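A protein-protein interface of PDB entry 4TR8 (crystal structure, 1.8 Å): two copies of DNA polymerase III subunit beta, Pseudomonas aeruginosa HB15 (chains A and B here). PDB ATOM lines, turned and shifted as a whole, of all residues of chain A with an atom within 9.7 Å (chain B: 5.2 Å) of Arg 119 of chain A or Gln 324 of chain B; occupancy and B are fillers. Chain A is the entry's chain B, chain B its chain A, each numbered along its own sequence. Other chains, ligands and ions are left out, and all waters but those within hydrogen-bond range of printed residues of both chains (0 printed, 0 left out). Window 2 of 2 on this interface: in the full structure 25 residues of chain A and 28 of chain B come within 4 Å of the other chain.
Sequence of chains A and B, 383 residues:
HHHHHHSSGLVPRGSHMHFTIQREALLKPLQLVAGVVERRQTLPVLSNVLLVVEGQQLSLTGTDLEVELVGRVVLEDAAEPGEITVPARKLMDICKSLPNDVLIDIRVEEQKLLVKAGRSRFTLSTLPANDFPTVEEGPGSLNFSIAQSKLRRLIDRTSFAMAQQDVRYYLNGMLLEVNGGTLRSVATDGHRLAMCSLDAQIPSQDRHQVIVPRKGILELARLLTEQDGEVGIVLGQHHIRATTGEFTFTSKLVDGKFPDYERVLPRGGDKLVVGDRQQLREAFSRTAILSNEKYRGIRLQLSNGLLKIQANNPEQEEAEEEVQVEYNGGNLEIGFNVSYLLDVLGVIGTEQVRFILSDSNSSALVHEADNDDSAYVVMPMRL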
ATOM      1  N   LEU A  98     -13.301  10.819  -7.183  1.00  0.00           N
ATOM      2  CA  LEU A  98     -12.963   9.617  -6.413  1.00  0.00           C
ATOM      3  C   LEU A  98     -13.879   8.433  -6.729  1.00  0.00           C
ATOM      4  O   LEU A  98     -15.030   8.666  -7.091  1.00  0.00           O
ATOM      5  CB  LEU A  98     -12.904   9.899  -4.889  1.00  0.00           C
ATOM      6  CG  LEU A  98     -11.709  10.748  -4.412  1.00  0.00           C
ATOM      7  CD1 LEU A  98     -11.950  11.286  -3.007  1.00  0.00           C
ATOM      8  CD2 LEU A  98     -10.388   9.984  -4.480  1.00  0.00           C
ATOM      9  N   PRO A  99     -13.391   7.168  -6.603  1.00  0.00           N
ATOM     10  CA  PRO A  99     -14.269   6.010  -6.864  1.00  0.00           C
ATOM     11  C   PRO A  99     -15.517   5.996  -5.977  1.00  0.00           C
ATOM     12  O   PRO A  99     -15.481   6.480  -4.834  1.00  0.00           O
ATOM     13  CB  PRO A  99     -13.379   4.808  -6.538  1.00  0.00           C
ATOM     14  CG  PRO A  99     -11.989   5.309  -6.617  1.00  0.00           C
ATOM     15  CD  PRO A  99     -12.045   6.732  -6.173  1.00  0.00           C
ATOM     16  N   VAL A 102     -16.200   5.067  -1.777  1.00  0.00           N
ATOM     17  CA  VAL A 102     -14.914   5.068  -1.072  1.00  0.00           C
ATOM     18  C   VAL A 102     -15.007   5.921   0.207  1.00  0.00           C
ATOM     19  O   VAL A 102     -15.693   6.949   0.223  1.00  0.00           O
ATOM     20  CB  VAL A 102     -13.698   5.451  -1.975  1.00  0.00           C
ATOM     21  CG1 VAL A 102     -13.578   6.963  -2.182  1.00  0.00           C
ATOM     22  CG2 VAL A 102     -12.396   4.882  -1.421  1.00  0.00           C
ATOM     23  N   LEU A 103     -14.311   5.489   1.260  1.00  0.00           N
ATOM     24  CA  LEU A 103     -14.242   6.225   2.518  1.00  0.00           C
ATOM     25  C   LEU A 103     -13.161   7.307   2.351  1.00  0.00           C
ATOM     26  O   LEU A 103     -12.051   7.016   1.882  1.00  0.00           O
ATOM     27  CB  LEU A 103     -13.908   5.265   3.684  1.00  0.00           C
ATOM     28  CG  LEU A 103     -13.981   5.825   5.114  1.00  0.00           C
ATOM     29  CD1 LEU A 103     -15.422   6.260   5.486  1.00  0.00           C
ATOM     30  CD2 LEU A 103     -13.498   4.797   6.109  1.00  0.00           C
ATOM     31  N   VAL A 115      -6.210  14.943   2.320  1.00  0.00           N
ATOM     32  CA  VAL A 115      -7.336  14.110   1.892  1.00  0.00           C
ATOM     33  C   VAL A 115      -6.783  12.751   1.442  1.00  0.00           C
ATOM     34  O   VAL A 115      -5.945  12.703   0.533  1.00  0.00           O
ATOM     35  CB  VAL A 115      -8.149  14.820   0.770  1.00  0.00           C
ATOM     36  CG1 VAL A 115      -9.243  13.913   0.189  1.00  0.00           C
ATOM     37  CG2 VAL A 115      -8.745  16.138   1.261  1.00  0.00           C
ATOM     38  N   LYS A 116      -7.236  11.662   2.094  1.00  0.00           N
ATOM     39  CA  LYS A 116      -6.832  10.291   1.745  1.00  0.00           C
ATOM     40  C   LYS A 116      -8.072   9.456   1.413  1.00  0.00           C
ATOM     41  O   LYS A 116      -9.065   9.517   2.137  1.00  0.00           O
ATOM     42  CB  LYS A 116      -6.032   9.625   2.886  1.00  0.00           C
ATOM     43  CG  LYS A 116      -4.717  10.323   3.233  1.00  0.00           C
ATOM     44  CD  LYS A 116      -3.935   9.570   4.307  1.00  0.00           C
ATOM     45  N   ALA A 117      -8.039   8.728   0.292  1.00  0.00           N
ATOM     46  CA  ALA A 117      -9.132   7.841  -0.137  1.00  0.00           C
ATOM     47  C   ALA A 117      -8.531   6.734  -1.005  1.00  0.00           C
ATOM     48  O   ALA A 117      -7.939   7.024  -2.051  1.00  0.00           O
ATOM     49  CB  ALA A 117     -10.194   8.619  -0.902  1.00  0.00           C
ATOM     50  N   GLY A 118      -8.633   5.490  -0.533  1.00  0.00           N
ATOM     51  CA  GLY A 118      -8.050   4.337  -1.209  1.00  0.00           C
ATOM     52  C   GLY A 118      -6.551   4.528  -1.342  1.00  0.00           C
ATOM     53  O   GLY A 118      -5.877   4.825  -0.356  1.00  0.00           O
ATOM     54  N   ARG A 119      -6.041   4.479  -2.587  1.00  0.00           N
ATOM     55  CA  ARG A 119      -4.613   4.676  -2.874  1.00  0.00           C
ATOM     56  C   ARG A 119      -4.290   6.147  -3.282  1.00  0.00           C
ATOM     57  O   ARG A 119      -3.204   6.407  -3.805  1.00  0.00           O
ATOM     58  CB  ARG A 119      -4.175   3.693  -3.999  1.00  0.00           C
ATOM     59  CG  ARG A 119      -4.076   2.237  -3.539  1.00  0.00           C
ATOM     60  CD  ARG A 119      -2.634   1.815  -3.358  1.00  0.00           C
ATOM     61  NE  ARG A 119      -2.415   0.440  -3.798  1.00  0.00           N
ATOM     62  CZ  ARG A 119      -1.220  -0.113  -3.966  1.00  0.00           C
ATOM     63  NH1 ARG A 119      -0.115   0.588  -3.734  1.00  0.00           N
ATOM     64  NH2 ARG A 119      -1.117  -1.370  -4.373  1.00  0.00           N
ATOM     65  N   SER A 120      -5.255   7.079  -3.100  1.00  0.00           N
ATOM     66  CA  SER A 120      -5.118   8.489  -3.482  1.00  0.00           C
ATOM     67  C   SER A 120      -4.842   9.369  -2.270  1.00  0.00           C
ATOM     68  O   SER A 120      -5.378   9.121  -1.182  1.00  0.00           O
ATOM     69  CB  SER A 120      -6.383   8.998  -4.179  1.00  0.00           C
ATOM     70  OG  SER A 120      -6.711   8.251  -5.337  1.00  0.00           O
ATOM     71  N   ARG A 121      -4.008  10.404  -2.476  1.00  0.00           N
ATOM     72  CA  ARG A 121      -3.647  11.398  -1.467  1.00  0.00           C
ATOM     73  C   ARG A 121      -3.669  12.799  -2.097  1.00  0.00           C
ATOM     74  O   ARG A 121      -3.192  12.984  -3.218  1.00  0.00           O
ATOM     75  CB  ARG A 121      -2.253  11.104  -0.863  1.00  0.00           C
ATOM     76  CG  ARG A 121      -2.226   9.921   0.106  1.00  0.00           C
ATOM     77  CD  ARG A 121      -0.808   9.510   0.475  1.00  0.00           C
ATOM     78  NE  ARG A 121      -0.141  10.512   1.312  1.00  0.00           N
ATOM     79  CZ  ARG A 121       0.054  10.394   2.622  1.00  0.00           C
ATOM     80  NH1 ARG A 121      -0.346   9.302   3.265  1.00  0.00           N
ATOM     81  NH2 ARG A 121       0.657  11.361   3.298  1.00  0.00           N
ATOM     82  N   PHE A 122      -4.215  13.779  -1.374  1.00  0.00           N
ATOM     83  CA  PHE A 122      -4.277  15.168  -1.835  1.00  0.00           C
ATOM     84  C   PHE A 122      -3.926  16.094  -0.674  1.00  0.00           C
ATOM     85  O   PHE A 122      -4.340  15.850   0.454  1.00  0.00           O
ATOM     86  CB  PHE A 122      -5.683  15.532  -2.362  1.00  0.00           C
ATOM     87  CG  PHE A 122      -6.202  14.612  -3.444  1.00  0.00           C
ATOM     88  CD1 PHE A 122      -6.862  13.432  -3.121  1.00  0.00           C
ATOM     89  CD2 PHE A 122      -6.036  14.930  -4.785  1.00  0.00           C
ATOM     90  CE1 PHE A 122      -7.323  12.571  -4.124  1.00  0.00           C
ATOM     91  CE2 PHE A 122      -6.503  14.072  -5.789  1.00  0.00           C
ATOM     92  CZ  PHE A 122      -7.147  12.904  -5.449  1.00  0.00           C
ATOM     93  N   GLY B 275      -1.128  -1.830 -18.004  1.00  0.00           N
ATOM     94  CA  GLY B 275      -1.997  -1.341 -16.942  1.00  0.00           C
ATOM     95  C   GLY B 275      -3.454  -1.307 -17.338  1.00  0.00           C
ATOM     96  O   GLY B 275      -3.791  -1.453 -18.519  1.00  0.00           O
ATOM     97  N   GLN B 279      -8.555   2.609 -15.047  1.00  0.00           N
ATOM     98  CA  GLN B 279      -7.937   2.919 -13.769  1.00  0.00           C
ATOM     99  C   GLN B 279      -6.840   3.981 -13.978  1.00  0.00           C
ATOM    100  O   GLN B 279      -6.787   4.957 -13.224  1.00  0.00           O
ATOM    101  CB  GLN B 279      -7.377   1.645 -13.118  1.00  0.00           C
ATOM    102  CG  GLN B 279      -6.825   1.939 -11.748  1.00  0.00           C
ATOM    103  CD  GLN B 279      -6.316   0.717 -11.046  1.00  0.00           C
ATOM    104  OE1 GLN B 279      -5.960  -0.298 -11.668  1.00  0.00           O
ATOM    105  NE2 GLN B 279      -6.190   0.843  -9.733  1.00  0.00           N
ATOM    106  N   GLY B 305       5.964  -3.737 -10.380  1.00  0.00           N
ATOM    107  CA  GLY B 305       4.522  -3.897 -10.232  1.00  0.00           C
ATOM    108  C   GLY B 305       3.756  -2.654  -9.812  1.00  0.00           C
ATOM    109  O   GLY B 305       2.595  -2.764  -9.408  1.00  0.00           O
ATOM    110  N   LEU B 306       4.391  -1.463  -9.888  1.00  0.00           N
ATOM    111  CA  LEU B 306       3.786  -0.250  -9.357  1.00  0.00           C
ATOM    112  C   LEU B 306       4.058   1.033 -10.123  1.00  0.00           C
ATOM    113  O   LEU B 306       5.190   1.324 -10.490  1.00  0.00           O
ATOM    114  CB  LEU B 306       4.298  -0.084  -7.899  1.00  0.00           C
ATOM    115  CG  LEU B 306       3.617   0.955  -7.019  1.00  0.00           C
ATOM    116  CD1 LEU B 306       2.160   0.530  -6.678  1.00  0.00           C
ATOM    117  CD2 LEU B 306       4.430   1.178  -5.747  1.00  0.00           C
ATOM    118  N   LEU B 307       3.013   1.853 -10.264  1.00  0.00           N
ATOM    119  CA  LEU B 307       3.136   3.166 -10.852  1.00  0.00           C
ATOM    120  C   LEU B 307       2.643   4.171  -9.818  1.00  0.00           C
ATOM    121  O   LEU B 307       1.506   4.065  -9.330  1.00  0.00           O
ATOM    122  CB  LEU B 307       2.323   3.282 -12.174  1.00  0.00           C
ATOM    123  CG  LEU B 307       2.100   4.729 -12.710  1.00  0.00           C
ATOM    124  CD1 LEU B 307       3.414   5.402 -13.108  1.00  0.00           C
ATOM    125  CD2 LEU B 307       1.176   4.727 -13.919  1.00  0.00           C
ATOM    126  N   GLU B 320      -1.243  12.587  -5.206  1.00  0.00           N
ATOM    127  CA  GLU B 320      -0.451  11.372  -5.416  1.00  0.00           C
ATOM    128  C   GLU B 320      -1.388  10.168  -5.508  1.00  0.00           C
ATOM    129  O   GLU B 320      -2.433  10.123  -4.843  1.00  0.00           O
ATOM    130  CB  GLU B 320       0.561  11.204  -4.266  1.00  0.00           C
ATOM    131  CG  GLU B 320       1.698  10.240  -4.536  1.00  0.00           C
ATOM    132  CD  GLU B 320       2.774  10.249  -3.462  1.00  0.00           C
ATOM    133  OE1 GLU B 320       3.971  10.308  -3.828  1.00  0.00           O
ATOM    134  OE2 GLU B 320       2.424  10.217  -2.258  1.00  0.00           O
ATOM    135  N   GLU B 321      -1.029   9.206  -6.357  1.00  0.00           N
ATOM    136  CA  GLU B 321      -1.833   8.005  -6.478  1.00  0.00           C
ATOM    137  C   GLU B 321      -0.954   6.855  -6.881  1.00  0.00           C
ATOM    138  O   GLU B 321      -0.112   7.008  -7.759  1.00  0.00           O
ATOM    139  CB  GLU B 321      -2.993   8.171  -7.473  1.00  0.00           C
ATOM    140  CG  GLU B 321      -4.051   7.094  -7.284  1.00  0.00           C
ATOM    141  CD  GLU B 321      -5.362   7.279  -8.020  1.00  0.00           C
ATOM    142  OE1 GLU B 321      -5.756   8.439  -8.272  1.00  0.00           O
ATOM    143  OE2 GLU B 321      -6.022   6.254  -8.299  1.00  0.00           O
ATOM    144  N   GLU B 322      -1.154   5.719  -6.249  1.00  0.00           N
ATOM    145  CA  GLU B 322      -0.434   4.491  -6.588  1.00  0.00           C
ATOM    146  C   GLU B 322      -1.373   3.576  -7.356  1.00  0.00           C
ATOM    147  O   GLU B 322      -2.522   3.367  -6.947  1.00  0.00           O
ATOM    148  CB  GLU B 322       0.103   3.796  -5.333  1.00  0.00           C
ATOM    149  CG  GLU B 322       1.175   4.593  -4.612  1.00  0.00           C
ATOM    150  CD  GLU B 322       1.785   3.903  -3.407  1.00  0.00           C
ATOM    151  OE1 GLU B 322       1.329   2.791  -3.053  1.00  0.00           O
ATOM    152  OE2 GLU B 322       2.725   4.479  -2.814  1.00  0.00           O
ATOM    153  N   VAL B 323      -0.902   3.068  -8.496  1.00  0.00           N
ATOM    154  CA  VAL B 323      -1.683   2.154  -9.335  1.00  0.00           C
ATOM    155  C   VAL B 323      -0.845   0.896  -9.582  1.00  0.00           C
ATOM    156  O   VAL B 323       0.323   1.006  -9.977  1.00  0.00           O
ATOM    157  CB  VAL B 323      -2.152   2.825 -10.666  1.00  0.00           C
ATOM    158  CG1 VAL B 323      -2.917   1.836 -11.553  1.00  0.00           C
ATOM    159  CG2 VAL B 323      -3.015   4.057 -10.388  1.00  0.00           C
ATOM    160  N   GLN B 324      -1.425  -0.286  -9.330  1.00  0.00           N
ATOM    161  CA  GLN B 324      -0.716  -1.540  -9.622  1.00  0.00           C
ATOM    162  C   GLN B 324      -0.703  -1.699 -11.142  1.00  0.00           C
ATOM    163  O   GLN B 324      -1.722  -1.472 -11.803  1.00  0.00           O
ATOM    164  CB  GLN B 324      -1.424  -2.750  -8.979  1.00  0.00           C
ATOM    165  CG  GLN B 324      -1.196  -2.863  -7.471  1.00  0.00           C
ATOM    166  CD  GLN B 324      -1.692  -4.184  -6.921  1.00  0.00           C
ATOM    167  OE1 GLN B 324      -2.679  -4.245  -6.179  1.00  0.00           O
ATOM    168  NE2 GLN B 324      -1.022  -5.276  -7.280  1.00  0.00           N
ATOM    169  N   VAL B 325       0.463  -2.033 -11.685  1.00  0.00           N
ATOM    170  CA  VAL B 325       0.679  -2.285 -13.123  1.00  0.00           C
ATOM    171  C   VAL B 325       1.546  -3.559 -13.286  1.00  0.00           C
ATOM    172  O   VAL B 325       2.266  -3.951 -12.365  1.00  0.00           O
ATOM    173  CB  VAL B 325       1.344  -1.080 -13.875  1.00  0.00           C
ATOM    174  CG1 VAL B 325       0.382   0.109 -14.005  1.00  0.00           C
ATOM    175  CG2 VAL B 325       2.681  -0.662 -13.239  1.00  0.00           C
ATOM    176  N   GLU B 326       1.513  -4.156 -14.473  1.00  0.00           N
ATOM    177  CA  GLU B 326       2.417  -5.257 -14.815  1.00  0.00           C
ATOM    178  C   GLU B 326       3.656  -4.534 -15.367  1.00  0.00           C
ATOM    179  O   GLU B 326       3.610  -3.949 -16.463  1.00  0.00           O
ATOM    180  CB  GLU B 326       1.804  -6.162 -15.885  1.00  0.00           C
ATOM    181  CG  GLU B 326       0.541  -6.894 -15.465  1.00  0.00           C
ATOM    182  CD  GLU B 326      -0.254  -7.499 -16.609  1.00  0.00           C
ATOM    183  OE1 GLU B 326       0.354  -7.882 -17.636  1.00  0.00           O
ATOM    184  OE2 GLU B 326      -1.495  -7.596 -16.472  1.00  0.00           O
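N of Glu 320 of chain B sits at hydrogen-bond distance from O of Arg 121 of chain A. The side-chain carboxylate (OE1) of Glu 321 of chain B sits at hydrogen-bond distance from the side-chain hydroxyl (OG) of Ser 120 of chain A, 3.1 Å away. The guanidinium group of Arg 119 of chain A is in salt-bridge range of the side-chain carboxylate of Glu 322 of chain B (2.7 Å).
Among the printed residues, merely in contact across the chains: Arg 119 of chain A with Glu 321 of chain B, Ser 120 of chain A with Glu 320 of chain B, Arg 119 of chain A with Gln 324 of chain B, Arg 119 of chain A with Leu 306 of chain B and Arg 119 of chain A with Glu 320 of chain B.
Of chain B, only Leu 306 (3.7 Å), Glu 320 (3.9 Å), Glu 321 (3.4 Å), Glu 322 (2.7 Å) and Gln 324 (3.4 Å) come within 4 Å of Arg 119 of chain A. Of chain A, only Arg 119 comes within 4 Å of Gln 324 of chain B. Val 323 of chain B touches none of the printed residues of chain A. No residue of chain A comes within 4 Å of Val 325 of chain B. Printed residues of chain B within 4 Å of Arg 121 of chain A: Glu 320. Of the printed residues of chain A, Glu 320 of chain B touches Arg 119 (3.9 Å), Ser 120 (3.4 Å) and Arg 121 (2.8 Å). Printed residues of chain B within 4 Å of Ser 120 of chain A: Glu 320 (3.4 Å) and Glu 321 (3.1 Å). Val 115 of chain A touches none of the printed residues of chain B.
Of the 12 printed residues of chain B, 5 touch a printed residue of chain A. Along chain B the printed residues that touch a printed residue of chain A span positions 306 to 324. Printed residues of chain A that touch a printed residue of chain B: Arg 119, Ser 120 and Arg 121. Among the printed residues, Asp or Glu carboxylates within 4 Å of a Lys or Arg side-chain nitrogen of the other chain: Arg 119 of chain A with Glu 322 of chain B.
No position is printed for both chains. Of the 8 pairs that touch across the chains among the printed residues, none has its exchanged pair printed and touching as well.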
